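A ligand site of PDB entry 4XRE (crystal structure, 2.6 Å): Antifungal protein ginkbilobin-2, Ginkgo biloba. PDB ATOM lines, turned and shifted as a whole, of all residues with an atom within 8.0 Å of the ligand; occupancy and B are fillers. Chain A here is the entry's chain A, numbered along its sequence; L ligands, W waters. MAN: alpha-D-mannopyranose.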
ATOM      1  N   SER A   9      12.500 -17.591 -20.364  1.00  0.00           N
ATOM      2  CA  SER A   9      12.803 -18.359 -21.564  1.00  0.00           C
ATOM      3  C   SER A   9      12.131 -19.737 -21.573  1.00  0.00           C
ATOM      4  O   SER A   9      11.823 -20.306 -20.533  1.00  0.00           O
ATOM      5  CB  SER A   9      14.319 -18.481 -21.803  1.00  0.00           C
ATOM      6  OG  SER A   9      14.921 -19.470 -20.975  1.00  0.00           O
ATOM      7  N   ALA A  10      11.885 -20.233 -22.786  1.00  0.00           N
ATOM      8  CA  ALA A  10      11.397 -21.590 -22.990  1.00  0.00           C
ATOM      9  C   ALA A  10      12.085 -22.189 -24.223  1.00  0.00           C
ATOM     10  O   ALA A  10      12.172 -21.543 -25.278  1.00  0.00           O
ATOM     11  CB  ALA A  10       9.897 -21.598 -23.162  1.00  0.00           C
ATOM     12  N   CYS A  11      12.568 -23.429 -24.080  1.00  0.00           N
ATOM     13  CA  CYS A  11      13.370 -24.080 -25.119  1.00  0.00           C
ATOM     14  C   CYS A  11      12.857 -25.470 -25.510  1.00  0.00           C
ATOM     15  O   CYS A  11      12.455 -26.261 -24.643  1.00  0.00           O
ATOM     16  CB  CYS A  11      14.832 -24.198 -24.646  1.00  0.00           C
ATOM     17  SG  CYS A  11      15.512 -22.714 -23.855  1.00  0.00           S
ATOM     18  N   ASN A  12      12.883 -25.775 -26.792  1.00  0.00           N
ATOM     19  CA  ASN A  12      12.615 -27.108 -27.260  1.00  0.00           C
ATOM     20  C   ASN A  12      13.634 -28.086 -26.734  1.00  0.00           C
ATOM     21  O   ASN A  12      14.789 -27.794 -26.720  1.00  0.00           O
ATOM     22  CB  ASN A  12      12.641 -27.107 -28.773  1.00  0.00           C
ATOM     23  CG  ASN A  12      11.855 -28.238 -29.374  1.00  0.00           C
ATOM     24  OD1 ASN A  12      12.042 -29.375 -29.056  1.00  0.00           O
ATOM     25  ND2 ASN A  12      10.976 -27.917 -30.282  1.00  0.00           N
ATOM     26  N   THR A  13      13.221 -29.265 -26.307  1.00  0.00           N
ATOM     27  CA  THR A  13      14.190 -30.269 -25.879  1.00  0.00           C
ATOM     28  C   THR A  13      15.031 -30.719 -27.075  1.00  0.00           C
ATOM     29  O   THR A  13      16.008 -31.458 -26.908  1.00  0.00           O
ATOM     30  CB  THR A  13      13.509 -31.497 -25.229  1.00  0.00           C
ATOM     31  OG1 THR A  13      12.510 -32.038 -26.107  1.00  0.00           O
ATOM     32  CG2 THR A  13      12.867 -31.084 -23.929  1.00  0.00           C
ATOM     33  N   GLN A  14      14.654 -30.262 -28.267  1.00  0.00           N
ATOM     34  CA  GLN A  14      15.283 -30.712 -29.515  1.00  0.00           C
ATOM     35  C   GLN A  14      16.148 -29.660 -30.215  1.00  0.00           C
ATOM     36  O   GLN A  14      15.712 -28.528 -30.472  1.00  0.00           O
ATOM     37  CB  GLN A  14      14.211 -31.242 -30.461  1.00  0.00           C
ATOM     38  CG  GLN A  14      14.751 -32.048 -31.597  1.00  0.00           C
ATOM     39  CD  GLN A  14      13.714 -32.983 -32.160  1.00  0.00           C
ATOM     40  OE1 GLN A  14      13.425 -34.020 -31.576  1.00  0.00           O
ATOM     41  NE2 GLN A  14      13.148 -32.611 -33.310  1.00  0.00           N
ATOM     42  N   CYS A  87      19.176 -21.076 -25.340  1.00  0.00           N
ATOM     43  CA  CYS A  87      18.495 -22.336 -25.616  1.00  0.00           C
ATOM     44  C   CYS A  87      19.370 -23.366 -26.338  1.00  0.00           C
ATOM     45  O   CYS A  87      18.880 -24.353 -26.879  1.00  0.00           O
ATOM     46  CB  CYS A  87      17.193 -22.089 -26.375  1.00  0.00           C
ATOM     47  SG  CYS A  87      15.870 -21.359 -25.337  1.00  0.00           S
ATOM     48  N   ALA A  90      18.386 -24.474 -30.371  1.00  0.00           N
ATOM     49  CA  ALA A  90      17.182 -25.286 -30.406  1.00  0.00           C
ATOM     50  C   ALA A  90      16.378 -25.107 -31.641  1.00  0.00           C
ATOM     51  O   ALA A  90      16.491 -24.132 -32.298  1.00  0.00           O
ATOM     52  CB  ALA A  90      16.320 -24.972 -29.226  1.00  0.00           C
ATOM     53  N   ILE A  91      15.527 -26.068 -31.921  1.00  0.00           N
ATOM     54  CA  ILE A  91      14.694 -25.994 -33.083  1.00  0.00           C
ATOM     55  C   ILE A  91      13.491 -25.120 -32.864  1.00  0.00           C
ATOM     56  O   ILE A  91      12.597 -25.135 -33.649  1.00  0.00           O
ATOM     57  CB  ILE A  91      14.194 -27.361 -33.544  1.00  0.00           C
ATOM     58  CG1 ILE A  91      13.124 -27.926 -32.598  1.00  0.00           C
ATOM     59  CG2 ILE A  91      15.347 -28.293 -33.719  1.00  0.00           C
ATOM     60  CD1 ILE A  91      12.369 -29.101 -33.150  1.00  0.00           C
ATOM     61  N   GLY A  92      13.481 -24.366 -31.790  1.00  0.00           N
ATOM     62  CA  GLY A  92      12.404 -23.458 -31.553  1.00  0.00           C
ATOM     63  C   GLY A  92      12.601 -22.773 -30.255  1.00  0.00           C
ATOM     64  O   GLY A  92      13.162 -23.321 -29.368  1.00  0.00           O
ATOM     65  N   ALA A  93      12.163 -21.550 -30.154  1.00  0.00           N
ATOM     66  CA  ALA A  93      12.344 -20.953 -28.838  1.00  0.00           C
ATOM     67  C   ALA A  93      11.612 -19.633 -28.683  1.00  0.00           C
ATOM     68  O   ALA A  93      11.337 -18.934 -29.647  1.00  0.00           O
ATOM     69  CB  ALA A  93      13.815 -20.764 -28.531  1.00  0.00           C
ATOM     70  N   ARG A  94      11.296 -19.315 -27.426  1.00  0.00           N
ATOM     71  CA  ARG A  94      10.795 -17.997 -27.047  1.00  0.00           C
ATOM     72  C   ARG A  94      11.785 -17.407 -26.061  1.00  0.00           C
ATOM     73  O   ARG A  94      12.286 -18.100 -25.191  1.00  0.00           O
ATOM     74  CB  ARG A  94       9.452 -18.119 -26.309  1.00  0.00           C
ATOM     75  CG  ARG A  94       8.263 -18.460 -27.185  1.00  0.00           C
ATOM     76  CD  ARG A  94       7.063 -18.859 -26.337  1.00  0.00           C
ATOM     77  NE  ARG A  94       7.174 -20.216 -25.811  1.00  0.00           N
ATOM     78  CZ  ARG A  94       6.328 -20.760 -24.940  1.00  0.00           C
ATOM     79  NH1 ARG A  94       5.299 -20.069 -24.479  1.00  0.00           N
ATOM     80  NH2 ARG A  94       6.522 -22.009 -24.529  1.00  0.00           N
ATOM     81  N   VAL A  95      12.054 -16.110 -26.193  1.00  0.00           N
ATOM     82  CA  VAL A  95      12.878 -15.416 -25.203  1.00  0.00           C
ATOM     83  C   VAL A  95      12.319 -14.051 -24.856  1.00  0.00           C
ATOM     84  O   VAL A  95      12.062 -13.229 -25.730  1.00  0.00           O
ATOM     85  CB  VAL A  95      14.332 -15.259 -25.655  1.00  0.00           C
ATOM     86  CG1 VAL A  95      15.050 -14.275 -24.752  1.00  0.00           C
ATOM     87  CG2 VAL A  95      15.031 -16.621 -25.661  1.00  0.00           C
ATOM     88  N   PHE A 101      10.929  -9.053 -27.301  1.00  0.00           N
ATOM     89  CA  PHE A 101      10.594 -10.478 -27.312  1.00  0.00           C
ATOM     90  C   PHE A 101      10.867 -11.067 -28.687  1.00  0.00           C
ATOM     91  O   PHE A 101      10.691 -10.404 -29.705  1.00  0.00           O
ATOM     92  CB  PHE A 101       9.122 -10.636 -26.945  1.00  0.00           C
ATOM     93  CG  PHE A 101       8.577 -12.024 -27.137  1.00  0.00           C
ATOM     94  CD1 PHE A 101       8.643 -12.948 -26.103  1.00  0.00           C
ATOM     95  CD2 PHE A 101       7.980 -12.390 -28.334  1.00  0.00           C
ATOM     96  CE1 PHE A 101       8.142 -14.218 -26.279  1.00  0.00           C
ATOM     97  CE2 PHE A 101       7.473 -13.657 -28.502  1.00  0.00           C
ATOM     98  CZ  PHE A 101       7.549 -14.575 -27.477  1.00  0.00           C
ATOM     99  N   ILE A 102      11.323 -12.307 -28.737  1.00  0.00           N
ATOM    100  CA  ILE A 102      11.434 -12.997 -29.998  1.00  0.00           C
ATOM    101  C   ILE A 102      11.006 -14.421 -29.820  1.00  0.00           C
ATOM    102  O   ILE A 102      11.283 -15.018 -28.781  1.00  0.00           O
ATOM    103  CB  ILE A 102      12.873 -13.041 -30.498  1.00  0.00           C
ATOM    104  CG1 ILE A 102      13.310 -11.669 -30.993  1.00  0.00           C
ATOM    105  CG2 ILE A 102      13.009 -14.041 -31.646  1.00  0.00           C
ATOM    106  CD1 ILE A 102      14.529 -11.730 -31.879  1.00  0.00           C
ATOM    107  N   GLN A 103      10.329 -14.982 -30.798  1.00  0.00           N
ATOM    108  CA  GLN A 103      10.094 -16.403 -30.783  1.00  0.00           C
ATOM    109  C   GLN A 103      10.338 -16.950 -32.164  1.00  0.00           C
ATOM    110  O   GLN A 103      10.087 -16.266 -33.157  1.00  0.00           O
ATOM    111  CB  GLN A 103       8.667 -16.731 -30.374  1.00  0.00           C
ATOM    112  CG  GLN A 103       8.342 -18.195 -30.596  1.00  0.00           C
ATOM    113  CD  GLN A 103       6.904 -18.521 -30.295  1.00  0.00           C
ATOM    114  OE1 GLN A 103       6.150 -17.653 -29.864  1.00  0.00           O
ATOM    115  NE2 GLN A 103       6.524 -19.767 -30.508  1.00  0.00           N
ATOM    116  N   TYR A 104      10.846 -18.168 -32.223  1.00  0.00           N
ATOM    117  CA  TYR A 104      10.969 -18.866 -33.498  1.00  0.00           C
ATOM    118  C   TYR A 104      10.631 -20.333 -33.320  1.00  0.00           C
ATOM    119  O   TYR A 104      10.854 -20.895 -32.261  1.00  0.00           O
ATOM    120  CB  TYR A 104      12.363 -18.697 -34.091  1.00  0.00           C
ATOM    121  CG  TYR A 104      13.487 -19.463 -33.420  1.00  0.00           C
ATOM    122  CD1 TYR A 104      13.692 -20.814 -33.692  1.00  0.00           C
ATOM    123  CD2 TYR A 104      14.378 -18.825 -32.570  1.00  0.00           C
ATOM    124  CE1 TYR A 104      14.733 -21.514 -33.097  1.00  0.00           C
ATOM    125  CE2 TYR A 104      15.432 -19.507 -31.973  1.00  0.00           C
ATOM    126  CZ  TYR A 104      15.607 -20.857 -32.242  1.00  0.00           C
ATOM    127  OH  TYR A 104      16.644 -21.546 -31.657  1.00  0.00           O
ATOM    128  N   GLU A 105      10.087 -20.937 -34.376  1.00  0.00           N
ATOM    129  CA  GLU A 105       9.653 -22.327 -34.348  1.00  0.00           C
ATOM    130  C   GLU A 105       9.720 -22.922 -35.738  1.00  0.00           C
ATOM    131  O   GLU A 105       9.882 -22.201 -36.728  1.00  0.00           O
ATOM    132  CB  GLU A 105       8.218 -22.414 -33.846  1.00  0.00           C
ATOM    133  CG  GLU A 105       7.927 -21.618 -32.594  1.00  0.00           C
ATOM    134  CD  GLU A 105       8.310 -22.353 -31.322  1.00  0.00           C
ATOM    135  OE1 GLU A 105       8.837 -23.476 -31.415  1.00  0.00           O
ATOM    136  OE2 GLU A 105       8.075 -21.805 -30.217  1.00  0.00           O
ATOM    137  N   GLN A 106       9.558 -24.241 -35.829  1.00  0.00           N
ATOM    138  CA  GLN A 106       9.593 -24.930 -37.112  1.00  0.00           C
ATOM    139  C   GLN A 106       8.200 -25.191 -37.709  1.00  0.00           C
ATOM    140  O   GLN A 106       8.069 -25.776 -38.794  1.00  0.00           O
ATOM    141  CB  GLN A 106      10.386 -26.228 -36.974  1.00  0.00           C
ATOM    142  CG  GLN A 106      11.838 -25.993 -36.638  1.00  0.00           C
ATOM    143  CD  GLN A 106      12.678 -27.248 -36.765  1.00  0.00           C
ATOM    144  OE1 GLN A 106      12.168 -28.362 -36.594  1.00  0.00           O
ATOM    145  NE2 GLN A 106      13.952 -27.079 -37.064  1.00  0.00           N
ATOM    146  N   ARG A 107       7.177 -24.769 -36.989  1.00  0.00           N
ATOM    147  CA  ARG A 107       5.814 -24.767 -37.530  1.00  0.00           C
ATOM    148  C   ARG A 107       5.239 -23.369 -37.354  1.00  0.00           C
ATOM    149  O   ARG A 107       5.914 -22.444 -36.935  1.00  0.00           O
ATOM    150  CB  ARG A 107       4.918 -25.744 -36.783  1.00  0.00           C
ATOM    151  CG  ARG A 107       5.643 -26.882 -36.083  1.00  0.00           C
ATOM    152  CD  ARG A 107       4.851 -27.325 -34.868  1.00  0.00           C
ATOM    153  NE  ARG A 107       4.416 -26.187 -34.071  1.00  0.00           N
ATOM    154  CZ  ARG A 107       3.900 -26.270 -32.842  1.00  0.00           C
ATOM    155  NH1 ARG A 107       3.755 -27.468 -32.264  1.00  0.00           N
ATOM    156  NH2 ARG A 107       3.538 -25.169 -32.190  1.00  0.00           N
ATOM    157  N   PHE A 109       2.598 -20.706 -35.525  1.00  0.00           N
ATOM    158  CA  PHE A 109       2.119 -20.511 -34.157  1.00  0.00           C
ATOM    159  C   PHE A 109       1.393 -19.175 -34.019  1.00  0.00           C
ATOM    160  O   PHE A 109       1.549 -18.277 -34.854  1.00  0.00           O
ATOM    161  CB  PHE A 109       3.279 -20.568 -33.167  1.00  0.00           C
ATOM    162  CG  PHE A 109       4.348 -19.545 -33.426  1.00  0.00           C
ATOM    163  CD1 PHE A 109       5.248 -19.723 -34.476  1.00  0.00           C
ATOM    164  CD2 PHE A 109       4.440 -18.406 -32.651  1.00  0.00           C
ATOM    165  CE1 PHE A 109       6.222 -18.774 -34.734  1.00  0.00           C
ATOM    166  CE2 PHE A 109       5.399 -17.459 -32.893  1.00  0.00           C
ATOM    167  CZ  PHE A 109       6.299 -17.638 -33.943  1.00  0.00           C
ATOM    168  OXT PHE A 109       0.632 -18.980 -33.058  1.00  0.00           O
HETATM  169  C1  MAN L   1       7.542 -25.316 -25.481  1.00  0.00           C
HETATM  170  C2  MAN L   1       6.820 -26.154 -26.562  1.00  0.00           C
HETATM  171  C3  MAN L   1       7.807 -26.463 -27.669  1.00  0.00           C
HETATM  172  C4  MAN L   1       8.292 -25.158 -28.243  1.00  0.00           C
HETATM  173  C5  MAN L   1       8.962 -24.362 -27.142  1.00  0.00           C
HETATM  174  C6  MAN L   1       9.458 -23.067 -27.743  1.00  0.00           C
HETATM  175  O1  MAN L   1       8.633 -26.098 -24.984  1.00  0.00           O
HETATM  176  O2  MAN L   1       5.695 -25.483 -27.129  1.00  0.00           O
HETATM  177  O3  MAN L   1       7.253 -27.322 -28.668  1.00  0.00           O
HETATM  178  O4  MAN L   1       9.259 -25.385 -29.255  1.00  0.00           O
HETATM  179  O5  MAN L   1       8.077 -24.123 -26.039  1.00  0.00           O
HETATM  180  O6  MAN L   1       8.476 -22.051 -27.695  1.00  0.00           O
HETATM  181  O   HOH W   1       6.049 -26.298 -30.754  1.00  0.00           O
HETATM  182  O   HOH W   2       7.327 -30.019 -29.441  1.00  0.00           O
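OE2 of Glu 105 sits at hydrogen-bond distance from O6 of the ligand. NE of Arg 94 sits at hydrogen-bond distance from O6 of the ligand (2.9 Å). ND2 of Asn 12 lies within hydrogen-bond range of O4 of the ligand (3.2 Å).
The side-chain carboxylate (OE2) of Glu 105 is in hydrogen-bond range of the side-chain amide nitrogen (NE2) of Gln 103. N of Arg 94 sits at hydrogen-bond distance from O of Ala 10, at 3.2 Å. The side-chain amide oxygen of Asn 12 lies close to the backbone NH of Gln 14 (2.9 Å). The backbone NH of Ala 93 is in hydrogen-bond range of the backbone carbonyl oxygen of Tyr 104 (2.6 Å). SG of Cys 87 is disulfide-bonded to SG of Cys 11, at 2.0 Å.
Ala 10 touches the ligand (O to C6, 3.97 Å). O of Cys 11 touches O1 of the ligand, 3.8 Å away. CA of Ala 93 touches C6 of the ligand (3.7 Å). Six residues have an atom within 4 Å of the ligand: Ala 10, Cys 11, Asn 12, Ala 93, Arg 94 and Glu 105.
Water W1 bridges O3 of the ligand and NH1 of Arg 107.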
